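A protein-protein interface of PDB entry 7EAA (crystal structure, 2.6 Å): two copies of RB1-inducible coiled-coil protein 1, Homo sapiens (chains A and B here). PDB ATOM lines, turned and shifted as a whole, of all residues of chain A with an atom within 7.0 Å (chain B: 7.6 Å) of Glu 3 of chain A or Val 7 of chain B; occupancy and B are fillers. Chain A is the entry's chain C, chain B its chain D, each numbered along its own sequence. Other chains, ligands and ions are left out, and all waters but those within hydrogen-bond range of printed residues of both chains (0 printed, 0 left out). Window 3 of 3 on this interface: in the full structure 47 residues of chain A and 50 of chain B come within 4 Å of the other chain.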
ATOM      1  N   GLY A   1       5.201   8.344  16.545  1.00  0.00           N
ATOM      2  CA  GLY A   1       5.073   9.716  17.005  1.00  0.00           C
ATOM      3  C   GLY A   1       3.779  10.398  16.589  1.00  0.00           C
ATOM      4  O   GLY A   1       2.802  10.398  17.346  1.00  0.00           O
ATOM      5  N   SER A   2       3.774  10.967  15.379  1.00  0.00           N
ATOM      6  CA  SER A   2       2.663  11.745  14.840  1.00  0.00           C
ATOM      7  C   SER A   2       1.567  10.847  14.257  1.00  0.00           C
ATOM      8  O   SER A   2       1.732   9.632  14.073  1.00  0.00           O
ATOM      9  CB  SER A   2       3.158  12.689  13.746  1.00  0.00           C
ATOM     10  OG  SER A   2       4.131  12.045  12.933  1.00  0.00           O
ATOM     11  N   GLU A   3       0.425  11.471  13.944  1.00  0.00           N
ATOM     12  CA  GLU A   3      -0.648  10.739  13.275  1.00  0.00           C
ATOM     13  C   GLU A   3      -0.168  10.187  11.937  1.00  0.00           C
ATOM     14  O   GLU A   3      -0.457   9.038  11.588  1.00  0.00           O
ATOM     15  CB  GLU A   3      -1.871  11.645  13.089  1.00  0.00           C
ATOM     16  CG  GLU A   3      -3.202  10.985  13.448  1.00  0.00           C
ATOM     17  CD  GLU A   3      -3.242  10.471  14.887  1.00  0.00           C
ATOM     18  OE1 GLU A   3      -3.951   9.468  15.150  1.00  0.00           O
ATOM     19  OE2 GLU A   3      -2.576  11.071  15.766  1.00  0.00           O
ATOM     20  N   PHE A   4       0.598  10.984  11.191  1.00  0.00           N
ATOM     21  CA  PHE A   4       1.128  10.522   9.919  1.00  0.00           C
ATOM     22  C   PHE A   4       2.083   9.354  10.107  1.00  0.00           C
ATOM     23  O   PHE A   4       2.067   8.401   9.325  1.00  0.00           O
ATOM     24  CB  PHE A   4       1.832  11.667   9.212  1.00  0.00           C
ATOM     25  CG  PHE A   4       2.437  11.277   7.917  1.00  0.00           C
ATOM     26  CD1 PHE A   4       1.666  11.255   6.768  1.00  0.00           C
ATOM     27  CD2 PHE A   4       3.773  10.908   7.846  1.00  0.00           C
ATOM     28  CE1 PHE A   4       2.217  10.886   5.567  1.00  0.00           C
ATOM     29  CE2 PHE A   4       4.330  10.532   6.656  1.00  0.00           C
ATOM     30  CZ  PHE A   4       3.550  10.524   5.510  1.00  0.00           C
ATOM     31  N   SER A   5       2.944   9.424  11.120  1.00  0.00           N
ATOM     32  CA  SER A   5       3.885   8.339  11.367  1.00  0.00           C
ATOM     33  C   SER A   5       3.165   7.042  11.720  1.00  0.00           C
ATOM     34  O   SER A   5       3.682   5.951  11.449  1.00  0.00           O
ATOM     35  CB  SER A   5       4.852   8.727  12.488  1.00  0.00           C
ATOM     36  OG  SER A   5       5.933   9.495  11.985  1.00  0.00           O
ATOM     37  N   LEU A   6       1.981   7.138  12.327  1.00  0.00           N
ATOM     38  CA  LEU A   6       1.204   5.939  12.615  1.00  0.00           C
ATOM     39  C   LEU A   6       0.672   5.306  11.336  1.00  0.00           C
ATOM     40  O   LEU A   6       0.777   4.083  11.156  1.00  0.00           O
ATOM     41  CB  LEU A   6       0.060   6.273  13.568  1.00  0.00           C
ATOM     42  CG  LEU A   6       0.531   6.619  14.982  1.00  0.00           C
ATOM     43  CD1 LEU A   6      -0.537   7.398  15.764  1.00  0.00           C
ATOM     44  CD2 LEU A   6       0.944   5.344  15.715  1.00  0.00           C
ATOM     45  N   VAL A   7       0.109   6.122  10.436  1.00  0.00           N
ATOM     46  CA  VAL A   7      -0.338   5.621   9.137  1.00  0.00           C
ATOM     47  C   VAL A   7       0.804   4.919   8.416  1.00  0.00           C
ATOM     48  O   VAL A   7       0.642   3.805   7.903  1.00  0.00           O
ATOM     49  CB  VAL A   7      -0.916   6.759   8.279  1.00  0.00           C
ATOM     50  CG1 VAL A   7      -1.398   6.216   6.954  1.00  0.00           C
ATOM     51  CG2 VAL A   7      -2.039   7.474   9.008  1.00  0.00           C
ATOM     52  N   ALA A   8       1.982   5.549   8.384  1.00  0.00           N
ATOM     53  CA  ALA A   8       3.129   4.915   7.746  1.00  0.00           C
ATOM     54  C   ALA A   8       3.467   3.573   8.403  1.00  0.00           C
ATOM     55  O   ALA A   8       3.687   2.573   7.706  1.00  0.00           O
ATOM     56  CB  ALA A   8       4.329   5.852   7.766  1.00  0.00           C
ATOM     57  N   LEU A  10       1.430   1.617  10.132  1.00  0.00           N
ATOM     58  CA  LEU A  10       0.343   0.682   9.878  1.00  0.00           C
ATOM     59  C   LEU A  10       0.403   0.118   8.467  1.00  0.00           C
ATOM     60  O   LEU A  10       0.134  -1.063   8.264  1.00  0.00           O
ATOM     61  CB  LEU A  10      -0.994   1.364  10.139  1.00  0.00           C
ATOM     62  CG  LEU A  10      -1.290   1.449  11.633  1.00  0.00           C
ATOM     63  CD1 LEU A  10      -2.367   2.492  11.923  1.00  0.00           C
ATOM     64  CD2 LEU A  10      -1.686   0.057  12.175  1.00  0.00           C
ATOM     65  N   SER B   5     -10.737   9.241  10.848  1.00  0.00           N
ATOM     66  CA  SER B   5      -9.353   8.900  11.175  1.00  0.00           C
ATOM     67  C   SER B   5      -8.791   7.741  10.337  1.00  0.00           C
ATOM     68  O   SER B   5      -9.257   6.601  10.422  1.00  0.00           O
ATOM     69  CB  SER B   5      -9.224   8.547  12.658  1.00  0.00           C
ATOM     70  OG  SER B   5      -7.854   8.499  13.042  1.00  0.00           O
ATOM     71  N   LEU B   6      -7.768   8.043   9.538  1.00  0.00           N
ATOM     72  CA  LEU B   6      -7.143   7.008   8.728  1.00  0.00           C
ATOM     73  C   LEU B   6      -6.395   5.998   9.596  1.00  0.00           C
ATOM     74  O   LEU B   6      -6.362   4.807   9.270  1.00  0.00           O
ATOM     75  CB  LEU B   6      -6.219   7.655   7.701  1.00  0.00           C
ATOM     76  CG  LEU B   6      -5.436   6.765   6.739  1.00  0.00           C
ATOM     77  CD1 LEU B   6      -6.352   5.831   5.965  1.00  0.00           C
ATOM     78  CD2 LEU B   6      -4.674   7.654   5.795  1.00  0.00           C
ATOM     79  N   VAL B   7      -5.799   6.460  10.699  1.00  0.00           N
ATOM     80  CA  VAL B   7      -5.168   5.555  11.650  1.00  0.00           C
ATOM     81  C   VAL B   7      -6.180   4.536  12.147  1.00  0.00           C
ATOM     82  O   VAL B   7      -5.905   3.328  12.189  1.00  0.00           O
ATOM     83  CB  VAL B   7      -4.556   6.349  12.816  1.00  0.00           C
ATOM     84  CG1 VAL B   7      -4.426   5.476  14.052  1.00  0.00           C
ATOM     85  CG2 VAL B   7      -3.213   6.910  12.421  1.00  0.00           C
ATOM     86  N   ALA B   8      -7.369   5.007  12.527  1.00  0.00           N
ATOM     87  CA  ALA B   8      -8.423   4.103  12.963  1.00  0.00           C
ATOM     88  C   ALA B   8      -8.707   3.053  11.895  1.00  0.00           C
ATOM     89  O   ALA B   8      -8.704   1.849  12.169  1.00  0.00           O
ATOM     90  CB  ALA B   8      -9.685   4.904  13.294  1.00  0.00           C
ATOM     91  N   GLU B   9      -8.920   3.502  10.654  1.00  0.00           N
ATOM     92  CA  GLU B   9      -9.294   2.588   9.580  1.00  0.00           C
ATOM     93  C   GLU B   9      -8.242   1.502   9.369  1.00  0.00           C
ATOM     94  O   GLU B   9      -8.580   0.329   9.177  1.00  0.00           O
ATOM     95  CB  GLU B   9      -9.521   3.384   8.296  1.00  0.00           C
ATOM     96  CG  GLU B   9     -10.225   2.644   7.169  1.00  0.00           C
ATOM     97  CD  GLU B   9      -9.718   3.076   5.791  1.00  0.00           C
ATOM     98  OE1 GLU B   9      -8.758   2.453   5.283  1.00  0.00           O
ATOM     99  OE2 GLU B   9     -10.259   4.059   5.228  1.00  0.00           O
ATOM    100  N   LEU B  10      -6.962   1.868   9.418  1.00  0.00           N
ATOM    101  CA  LEU B  10      -5.899   0.895   9.204  1.00  0.00           C
ATOM    102  C   LEU B  10      -5.710  -0.019  10.407  1.00  0.00           C
ATOM    103  O   LEU B  10      -5.360  -1.193  10.239  1.00  0.00           O
ATOM    104  CB  LEU B  10      -4.591   1.616   8.858  1.00  0.00           C
ATOM    105  CG  LEU B  10      -4.621   2.377   7.527  1.00  0.00           C
ATOM    106  CD1 LEU B  10      -3.394   3.232   7.355  1.00  0.00           C
ATOM    107  CD2 LEU B  10      -4.753   1.425   6.365  1.00  0.00           C
ATOM    108  N   GLN B  11      -5.941   0.494  11.618  1.00  0.00           N
ATOM    109  CA  GLN B  11      -5.946  -0.372  12.791  1.00  0.00           C
ATOM    110  C   GLN B  11      -7.011  -1.450  12.659  1.00  0.00           C
ATOM    111  O   GLN B  11      -6.750  -2.631  12.932  1.00  0.00           O
ATOM    112  CB  GLN B  11      -6.146   0.449  14.059  1.00  0.00           C
ATOM    113  CG  GLN B  11      -4.840   0.986  14.620  1.00  0.00           C
ATOM    114  CD  GLN B  11      -5.032   2.117  15.631  1.00  0.00           C
ATOM    115  OE1 GLN B  11      -6.143   2.622  15.828  1.00  0.00           O
ATOM    116  NE2 GLN B  11      -3.936   2.523  16.272  1.00  0.00           N
ATOM    117  N   GLU B  12      -8.200  -1.078  12.180  1.00  0.00           N
ATOM    118  CA  GLU B  12      -9.236  -2.086  11.980  1.00  0.00           C
ATOM    119  C   GLU B  12      -8.911  -3.025  10.814  1.00  0.00           C
ATOM    120  O   GLU B  12      -9.043  -4.248  10.949  1.00  0.00           O
ATOM    121  CB  GLU B  12     -10.594  -1.413  11.798  1.00  0.00           C
ATOM    122  CG  GLU B  12     -11.290  -1.090  13.130  1.00  0.00           C
ATOM    123  CD  GLU B  12     -10.833   0.238  13.768  1.00  0.00           C
ATOM    124  OE1 GLU B  12      -9.974   0.204  14.678  1.00  0.00           O
ATOM    125  OE2 GLU B  12     -11.338   1.315  13.363  1.00  0.00           O
ATOM    126  N   LYS B  13      -8.478  -2.486   9.672  1.00  0.00           N
ATOM    127  CA  LYS B  13      -8.172  -3.345   8.532  1.00  0.00           C
ATOM    128  C   LYS B  13      -7.040  -4.314   8.843  1.00  0.00           C
ATOM    129  O   LYS B  13      -7.029  -5.431   8.323  1.00  0.00           O
ATOM    130  CB  LYS B  13      -7.828  -2.517   7.292  1.00  0.00           C
ATOM    131  CG  LYS B  13      -7.607  -3.358   6.015  1.00  0.00           C
ATOM    132  CD  LYS B  13      -8.851  -3.387   5.103  1.00  0.00           C
ATOM    133  CE  LYS B  13      -8.595  -4.087   3.745  1.00  0.00           C
ATOM    134  NZ  LYS B  13      -7.411  -3.577   2.952  1.00  0.00           N
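Among the printed residues, pairs that only touch across the chains: Leu 6 of chain A with Val 7 of chain B, Glu 3 of chain A with Val 7 of chain B, Val 7 of chain A with Leu 10 of chain B, Leu 10 of chain A with Val 7 of chain B, Val 7 of chain A with Val 7 of chain B, Val 7 of chain A with Leu 6 of chain B, Leu 10 of chain A with Leu 10 of chain B and Leu 10 of chain A with Gln 11 of chain B.
Leu 6 of chain A touches Val 7 of chain B, and with the chains exchanged Val 7 of chain A touches Leu 6 of chain B.
Val 7 of chain A touches its own counterpart, Val 7 of chain B.
Val 7 of chain A touches Leu 10 of chain B, and with the chains exchanged Leu 10 of chain A touches Val 7 of chain B.
Leu 10 of chain A touches its own counterpart, Leu 10 of chain B.
Positions printed for both chains: 5, 6, 7, 8 and 10.
Of chain B, only Val 7 (3.6 Å) comes within 4 Å of Glu 3 of chain A.
Of chain A, only Glu 3 (3.6 Å), Leu 6 (3.5 Å), Val 7 (3.7 Å) and Leu 10 (3.6 Å) come within 4 Å of Val 7 of chain B.
Printed residues of chain A within 4 Å of Leu 10 of chain B: Val 7 and Leu 10.
Of the printed residues of chain A, Gln 11 of chain B touches Leu 10 (3.96 Å).
Of the printed residues of chain B, Val 7 of chain A touches Leu 6, Val 7 and Leu 10.
Ser 2 of chain A touches none of the printed residues of chain B.
The nearest residue of chain A that does not touch Val 7 of chain B is Phe 4 of chain A (5.7 Å).
The nearest printed residue of chain B that does not touch Leu 6 of chain A is Gln 11 of chain B (5.7 Å).
Of the 9 printed residues of chain B, 4 touch a printed residue of chain A.
Hydrophobic or aromatic side chains of chain B within 4 Å of the printed part of chain A: Leu 6, Val 7 and Leu 10.
Printed residues of chain A that touch a printed residue of chain B: Glu 3, Leu 6, Val 7 and Leu 10.
Hydrophobic or aromatic side chains of chain A that line the printed part of chain B: Leu 6, Val 7 and Leu 10.
Among the printed residues, 8 pairs touch across the chains.
Among the printed residues, no Asp or Glu carboxylate lies within 4 Å of a Lys or Arg side-chain nitrogen of the other chain.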
